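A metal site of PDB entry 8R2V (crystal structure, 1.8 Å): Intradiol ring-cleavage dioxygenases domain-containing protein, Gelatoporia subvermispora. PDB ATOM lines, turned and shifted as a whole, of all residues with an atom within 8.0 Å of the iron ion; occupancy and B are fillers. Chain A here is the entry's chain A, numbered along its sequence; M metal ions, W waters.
The backbone carbonyl oxygen (O) of Tyr 211 is in hydrogen-bond range of the backbone NH (N) of Arg 232 (2.9 Å).
NH1 of Arg 232 lies close to NE2 of His 235 (3.3 Å).
The backbone carbonyl oxygen of Pro 233 is in hydrogen-bond range of a ring nitrogen (ND1) of His 235 (2.7 Å).
The backbone carbonyl oxygen (O) of Trp 169 is in hydrogen-bond range of the backbone NH (N) of His 237 (3.0 Å).
Of the 23 residues printed, 4 come within 4 Å of the iron ion.
The iron ion is bound by the side-chain hydroxyl (OH) of Tyr 177 (1.9 Å), the side-chain hydroxyl (OH) of Tyr 211 (2.1 Å), a ring nitrogen (NE2) of His 235 (2.1 Å), water W1 (2.1 Å) and a ring nitrogen (NE2) of His 237 (2.2 Å).
The iron ion has five donor atoms within binding distance.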
ATOM      1  N   VAL A 120       0.372   5.170  21.304  1.00  0.00           N
ATOM      2  CA  VAL A 120      -0.559   6.083  21.971  1.00  0.00           C
ATOM      3  C   VAL A 120       0.010   6.540  23.317  1.00  0.00           C
ATOM      4  O   VAL A 120       0.739   5.818  23.984  1.00  0.00           O
ATOM      5  CB  VAL A 120      -1.930   5.385  22.109  1.00  0.00           C
ATOM      6  CG1 VAL A 120      -2.561   5.130  20.731  1.00  0.00           C
ATOM      7  CG2 VAL A 120      -1.843   4.094  22.901  1.00  0.00           C
ATOM      8  N   LEU A 121      -0.335   7.775  23.716  1.00  0.00           N
ATOM      9  CA  LEU A 121       0.178   8.418  24.908  1.00  0.00           C
ATOM     10  C   LEU A 121      -0.474   7.842  26.179  1.00  0.00           C
ATOM     11  O   LEU A 121       0.199   7.702  27.229  1.00  0.00           O
ATOM     12  CB  LEU A 121      -0.142   9.908  24.811  1.00  0.00           C
ATOM     13  CG  LEU A 121       0.233  10.742  26.022  1.00  0.00           C
ATOM     14  CD1 LEU A 121       1.744  10.893  26.120  1.00  0.00           C
ATOM     15  CD2 LEU A 121      -0.441  12.116  25.979  1.00  0.00           C
ATOM     16  N   GLY A 122      -1.798   7.615  26.081  1.00  0.00           N
ATOM     17  CA  GLY A 122      -2.647   7.309  27.222  1.00  0.00           C
ATOM     18  C   GLY A 122      -2.792   8.494  28.183  1.00  0.00           C
ATOM     19  O   GLY A 122      -2.252   9.582  27.981  1.00  0.00           O
ATOM     20  N   PRO A 123      -3.506   8.305  29.295  1.00  0.00           N
ATOM     21  CA  PRO A 123      -3.769   9.418  30.214  1.00  0.00           C
ATOM     22  C   PRO A 123      -2.823   9.665  31.386  1.00  0.00           C
ATOM     23  O   PRO A 123      -3.156  10.488  32.252  1.00  0.00           O
ATOM     24  CB  PRO A 123      -5.129   8.973  30.833  1.00  0.00           C
ATOM     25  CG  PRO A 123      -5.015   7.452  30.887  1.00  0.00           C
ATOM     26  CD  PRO A 123      -4.211   7.053  29.648  1.00  0.00           C
ATOM     27  N   PHE A 124      -1.704   8.915  31.478  1.00  0.00           N
ATOM     28  CA  PHE A 124      -0.943   8.924  32.728  1.00  0.00           C
ATOM     29  C   PHE A 124       0.318   9.800  32.648  1.00  0.00           C
ATOM     30  O   PHE A 124       1.142   9.756  33.566  1.00  0.00           O
ATOM     31  CB  PHE A 124      -0.681   7.479  33.154  1.00  0.00           C
ATOM     32  CG  PHE A 124      -1.959   6.797  33.568  1.00  0.00           C
ATOM     33  CD1 PHE A 124      -2.663   7.207  34.696  1.00  0.00           C
ATOM     34  CD2 PHE A 124      -2.487   5.748  32.825  1.00  0.00           C
ATOM     35  CE1 PHE A 124      -3.832   6.557  35.092  1.00  0.00           C
ATOM     36  CE2 PHE A 124      -3.650   5.104  33.218  1.00  0.00           C
ATOM     37  CZ  PHE A 124      -4.328   5.529  34.335  1.00  0.00           C
ATOM     38  N   PHE A 125       0.445  10.610  31.591  1.00  0.00           N
ATOM     39  CA  PHE A 125       1.590  11.498  31.519  1.00  0.00           C
ATOM     40  C   PHE A 125       1.359  12.637  32.529  1.00  0.00           C
ATOM     41  O   PHE A 125       0.245  13.101  32.702  1.00  0.00           O
ATOM     42  CB  PHE A 125       1.795  11.985  30.070  1.00  0.00           C
ATOM     43  CG  PHE A 125       2.851  13.047  29.975  1.00  0.00           C
ATOM     44  CD1 PHE A 125       4.184  12.740  30.186  1.00  0.00           C
ATOM     45  CD2 PHE A 125       2.504  14.385  29.806  1.00  0.00           C
ATOM     46  CE1 PHE A 125       5.159  13.727  30.190  1.00  0.00           C
ATOM     47  CE2 PHE A 125       3.469  15.376  29.793  1.00  0.00           C
ATOM     48  CZ  PHE A 125       4.809  15.042  29.984  1.00  0.00           C
ATOM     49  N   TRP A 169       7.414   6.888  31.962  1.00  0.00           N
ATOM     50  CA  TRP A 169       6.521   6.536  33.048  1.00  0.00           C
ATOM     51  C   TRP A 169       5.988   5.134  32.818  1.00  0.00           C
ATOM     52  O   TRP A 169       6.001   4.627  31.700  1.00  0.00           O
ATOM     53  CB  TRP A 169       5.389   7.589  33.215  1.00  0.00           C
ATOM     54  CG  TRP A 169       4.463   7.748  32.053  1.00  0.00           C
ATOM     55  CD1 TRP A 169       3.158   7.325  32.011  1.00  0.00           C
ATOM     56  CD2 TRP A 169       4.701   8.419  30.793  1.00  0.00           C
ATOM     57  NE1 TRP A 169       2.586   7.648  30.814  1.00  0.00           N
ATOM     58  CE2 TRP A 169       3.509   8.309  30.035  1.00  0.00           C
ATOM     59  CE3 TRP A 169       5.787   9.094  30.229  1.00  0.00           C
ATOM     60  CZ2 TRP A 169       3.388   8.812  28.743  1.00  0.00           C
ATOM     61  CZ3 TRP A 169       5.672   9.591  28.932  1.00  0.00           C
ATOM     62  CH2 TRP A 169       4.485   9.460  28.213  1.00  0.00           C
ATOM     63  N   GLU A 170       5.523   4.525  33.912  1.00  0.00           N
ATOM     64  CA  GLU A 170       5.041   3.149  33.866  1.00  0.00           C
ATOM     65  C   GLU A 170       4.292   2.836  35.147  1.00  0.00           C
ATOM     66  O   GLU A 170       4.391   3.582  36.111  1.00  0.00           O
ATOM     67  CB  GLU A 170       6.213   2.157  33.792  1.00  0.00           C
ATOM     68  CG  GLU A 170       7.163   2.265  34.981  1.00  0.00           C
ATOM     69  CD  GLU A 170       8.259   1.196  35.060  1.00  0.00           C
ATOM     70  OE1 GLU A 170       9.252   1.415  35.797  1.00  0.00           O
ATOM     71  OE2 GLU A 170       8.112   0.140  34.398  1.00  0.00           O
ATOM     72  N   THR A 171       3.613   1.701  35.150  1.00  0.00           N
ATOM     73  CA  THR A 171       3.007   1.161  36.357  1.00  0.00           C
ATOM     74  C   THR A 171       4.055   0.625  37.313  1.00  0.00           C
ATOM     75  O   THR A 171       5.186   0.345  36.924  1.00  0.00           O
ATOM     76  CB  THR A 171       2.073  -0.013  36.064  1.00  0.00           C
ATOM     77  OG1 THR A 171       2.863  -1.126  35.632  1.00  0.00           O
ATOM     78  CG2 THR A 171       1.032   0.388  35.056  1.00  0.00           C
ATOM     79  N   TYR A 177      -0.377   3.368  38.092  1.00  0.00           N
ATOM     80  CA  TYR A 177       0.404   4.594  37.970  1.00  0.00           C
ATOM     81  C   TYR A 177       0.282   5.387  39.270  1.00  0.00           C
ATOM     82  O   TYR A 177      -0.611   5.143  40.078  1.00  0.00           O
ATOM     83  CB  TYR A 177      -0.033   5.439  36.775  1.00  0.00           C
ATOM     84  CG  TYR A 177       0.229   4.809  35.430  1.00  0.00           C
ATOM     85  CD1 TYR A 177      -0.693   3.972  34.814  1.00  0.00           C
ATOM     86  CD2 TYR A 177       1.463   4.976  34.804  1.00  0.00           C
ATOM     87  CE1 TYR A 177      -0.430   3.367  33.588  1.00  0.00           C
ATOM     88  CE2 TYR A 177       1.736   4.376  33.584  1.00  0.00           C
ATOM     89  CZ  TYR A 177       0.805   3.561  32.966  1.00  0.00           C
ATOM     90  OH  TYR A 177       1.075   2.977  31.740  1.00  0.00           O
ATOM     91  N   PRO A 208       7.153  -3.360  33.955  1.00  0.00           N
ATOM     92  CA  PRO A 208       5.751  -2.928  34.024  1.00  0.00           C
ATOM     93  C   PRO A 208       4.855  -4.143  33.842  1.00  0.00           C
ATOM     94  O   PRO A 208       5.323  -5.193  33.412  1.00  0.00           O
ATOM     95  CB  PRO A 208       5.629  -1.944  32.870  1.00  0.00           C
ATOM     96  CG  PRO A 208       6.613  -2.501  31.839  1.00  0.00           C
ATOM     97  CD  PRO A 208       7.780  -3.047  32.671  1.00  0.00           C
ATOM     98  N   VAL A 209       3.573  -4.003  34.183  1.00  0.00           N
ATOM     99  CA  VAL A 209       2.632  -5.103  34.058  1.00  0.00           C
ATOM    100  C   VAL A 209       1.358  -4.647  33.336  1.00  0.00           C
ATOM    101  O   VAL A 209       1.030  -3.453  33.256  1.00  0.00           O
ATOM    102  CB  VAL A 209       2.264  -5.698  35.437  1.00  0.00           C
ATOM    103  CG1 VAL A 209       3.482  -6.214  36.201  1.00  0.00           C
ATOM    104  CG2 VAL A 209       1.498  -4.715  36.281  1.00  0.00           C
ATOM    105  N   TYR A 211      -2.594  -3.979  32.573  1.00  0.00           N
ATOM    106  CA  TYR A 211      -3.593  -3.317  33.402  1.00  0.00           C
ATOM    107  C   TYR A 211      -4.831  -2.946  32.610  1.00  0.00           C
ATOM    108  O   TYR A 211      -4.793  -2.850  31.385  1.00  0.00           O
ATOM    109  CB  TYR A 211      -2.971  -2.074  34.061  1.00  0.00           C
ATOM    110  CG  TYR A 211      -2.566  -1.002  33.099  1.00  0.00           C
ATOM    111  CD1 TYR A 211      -3.515  -0.144  32.566  1.00  0.00           C
ATOM    112  CD2 TYR A 211      -1.231  -0.861  32.690  1.00  0.00           C
ATOM    113  CE1 TYR A 211      -3.159   0.837  31.659  1.00  0.00           C
ATOM    114  CE2 TYR A 211      -0.875   0.139  31.799  1.00  0.00           C
ATOM    115  CZ  TYR A 211      -1.840   0.974  31.281  1.00  0.00           C
ATOM    116  OH  TYR A 211      -1.560   1.925  30.364  1.00  0.00           O
ATOM    117  N   ILE A 213      -7.925  -0.473  31.297  1.00  0.00           N
ATOM    118  CA  ILE A 213      -8.408   0.865  31.040  1.00  0.00           C
ATOM    119  C   ILE A 213      -9.812   0.988  31.629  1.00  0.00           C
ATOM    120  O   ILE A 213     -10.431  -0.016  31.958  1.00  0.00           O
ATOM    121  CB  ILE A 213      -8.410   1.165  29.541  1.00  0.00           C
ATOM    122  CG1 ILE A 213      -9.392   0.259  28.795  1.00  0.00           C
ATOM    123  CG2 ILE A 213      -6.989   1.066  28.982  1.00  0.00           C
ATOM    124  CD1 ILE A 213      -9.558   0.612  27.337  1.00  0.00           C
ATOM    125  N   ARG A 232      -4.664  -3.556  28.609  1.00  0.00           N
ATOM    126  CA  ARG A 232      -3.448  -3.250  27.881  1.00  0.00           C
ATOM    127  C   ARG A 232      -2.333  -4.224  28.314  1.00  0.00           C
ATOM    128  O   ARG A 232      -2.183  -4.525  29.491  1.00  0.00           O
ATOM    129  CB  ARG A 232      -2.994  -1.835  28.191  1.00  0.00           C
ATOM    130  CG  ARG A 232      -3.995  -0.758  27.750  1.00  0.00           C
ATOM    131  CD  ARG A 232      -3.264   0.504  27.374  1.00  0.00           C
ATOM    132  NE  ARG A 232      -2.471   0.241  26.179  1.00  0.00           N
ATOM    133  CZ  ARG A 232      -1.453   0.979  25.744  1.00  0.00           C
ATOM    134  NH1 ARG A 232      -1.078   2.044  26.399  1.00  0.00           N
ATOM    135  NH2 ARG A 232      -0.800   0.638  24.644  1.00  0.00           N
ATOM    136  N   PRO A 233      -1.474  -4.728  27.395  1.00  0.00           N
ATOM    137  CA  PRO A 233      -0.285  -5.472  27.797  1.00  0.00           C
ATOM    138  C   PRO A 233       0.741  -4.511  28.403  1.00  0.00           C
ATOM    139  O   PRO A 233       0.628  -3.270  28.262  1.00  0.00           O
ATOM    140  CB  PRO A 233       0.244  -6.021  26.472  1.00  0.00           C
ATOM    141  CG  PRO A 233      -0.127  -4.919  25.487  1.00  0.00           C
ATOM    142  CD  PRO A 233      -1.503  -4.457  25.951  1.00  0.00           C
ATOM    143  N   ASN A 234       1.706  -5.113  29.126  1.00  0.00           N
ATOM    144  CA  ASN A 234       2.769  -4.402  29.804  1.00  0.00           C
ATOM    145  C   ASN A 234       3.447  -3.436  28.823  1.00  0.00           C
ATOM    146  O   ASN A 234       3.691  -3.788  27.678  1.00  0.00           O
ATOM    147  CB  ASN A 234       3.767  -5.386  30.437  1.00  0.00           C
ATOM    148  CG  ASN A 234       4.345  -6.463  29.538  1.00  0.00           C
ATOM    149  OD1 ASN A 234       4.924  -7.422  30.035  1.00  0.00           O
ATOM    150  ND2 ASN A 234       4.281  -6.317  28.217  1.00  0.00           N
ATOM    151  N   HIS A 235       3.790  -2.246  29.289  1.00  0.00           N
ATOM    152  CA  HIS A 235       4.594  -1.339  28.495  1.00  0.00           C
ATOM    153  C   HIS A 235       5.298  -0.300  29.371  1.00  0.00           C
ATOM    154  O   HIS A 235       4.829   0.061  30.455  1.00  0.00           O
ATOM    155  CB  HIS A 235       3.728  -0.607  27.454  1.00  0.00           C
ATOM    156  CG  HIS A 235       2.535   0.061  28.043  1.00  0.00           C
ATOM    157  ND1 HIS A 235       1.388  -0.650  28.311  1.00  0.00           N
ATOM    158  CD2 HIS A 235       2.303   1.351  28.459  1.00  0.00           C
ATOM    159  CE1 HIS A 235       0.493   0.193  28.864  1.00  0.00           C
ATOM    160  NE2 HIS A 235       1.012   1.432  28.944  1.00  0.00           N
ATOM    161  N   LEU A 236       6.387   0.241  28.791  1.00  0.00           N
ATOM    162  CA  LEU A 236       7.099   1.399  29.316  1.00  0.00           C
ATOM    163  C   LEU A 236       6.870   2.560  28.357  1.00  0.00           C
ATOM    164  O   LEU A 236       7.181   2.431  27.183  1.00  0.00           O
ATOM    165  CB  LEU A 236       8.601   1.064  29.360  1.00  0.00           C
ATOM    166  CG  LEU A 236       9.522   2.191  29.824  1.00  0.00           C
ATOM    167  CD1 LEU A 236       9.292   2.572  31.278  1.00  0.00           C
ATOM    168  CD2 LEU A 236      10.963   1.782  29.588  1.00  0.00           C
ATOM    169  N   HIS A 237       6.344   3.679  28.877  1.00  0.00           N
ATOM    170  CA  HIS A 237       6.122   4.852  28.067  1.00  0.00           C
ATOM    171  C   HIS A 237       7.402   5.682  27.991  1.00  0.00           C
ATOM    172  O   HIS A 237       8.132   5.806  28.980  1.00  0.00           O
ATOM    173  CB  HIS A 237       5.062   5.805  28.661  1.00  0.00           C
ATOM    174  CG  HIS A 237       3.685   5.246  28.645  1.00  0.00           C
ATOM    175  ND1 HIS A 237       2.809   5.393  27.590  1.00  0.00           N
ATOM    176  CD2 HIS A 237       2.992   4.566  29.641  1.00  0.00           C
ATOM    177  CE1 HIS A 237       1.650   4.800  27.933  1.00  0.00           C
ATOM    178  NE2 HIS A 237       1.748   4.299  29.169  1.00  0.00           N
ATOM    179  N   ALA A 251       6.147   3.711  23.166  1.00  0.00           N
ATOM    180  CA  ALA A 251       6.161   2.770  24.272  1.00  0.00           C
ATOM    181  C   ALA A 251       6.815   1.486  23.789  1.00  0.00           C
ATOM    182  O   ALA A 251       6.701   1.138  22.620  1.00  0.00           O
ATOM    183  CB  ALA A 251       4.776   2.514  24.836  1.00  0.00           C
ATOM    184  N   TYR A 253       6.965  -2.680  24.602  1.00  0.00           N
ATOM    185  CA  TYR A 253       6.058  -3.699  25.096  1.00  0.00           C
ATOM    186  C   TYR A 253       6.823  -5.005  25.311  1.00  0.00           C
ATOM    187  O   TYR A 253       7.140  -5.700  24.361  1.00  0.00           O
ATOM    188  CB  TYR A 253       4.909  -3.910  24.100  1.00  0.00           C
ATOM    189  CG  TYR A 253       4.091  -2.661  23.858  1.00  0.00           C
ATOM    190  CD1 TYR A 253       4.498  -1.698  22.954  1.00  0.00           C
ATOM    191  CD2 TYR A 253       2.924  -2.424  24.581  1.00  0.00           C
ATOM    192  CE1 TYR A 253       3.722  -0.574  22.712  1.00  0.00           C
ATOM    193  CE2 TYR A 253       2.163  -1.285  24.380  1.00  0.00           C
ATOM    194  CZ  TYR A 253       2.548  -0.358  23.435  1.00  0.00           C
ATOM    195  OH  TYR A 253       1.812   0.801  23.236  1.00  0.00           O
ATOM    196  N   VAL A 265      -6.343  -0.627  23.063  1.00  0.00           N
ATOM    197  CA  VAL A 265      -6.188   0.678  22.408  1.00  0.00           C
ATOM    198  C   VAL A 265      -5.187   0.650  21.237  1.00  0.00           C
ATOM    199  O   VAL A 265      -4.838   1.715  20.707  1.00  0.00           O
ATOM    200  CB  VAL A 265      -5.803   1.773  23.410  1.00  0.00           C
ATOM    201  CG1 VAL A 265      -6.841   1.914  24.518  1.00  0.00           C
ATOM    202  CG2 VAL A 265      -4.413   1.613  24.032  1.00  0.00           C
HETATM  203 FE    FE M   1       0.209   3.037  30.088  1.00  0.00          FE
HETATM  204  O   HOH W   1      -1.124   4.649  29.652  1.00  0.00           O
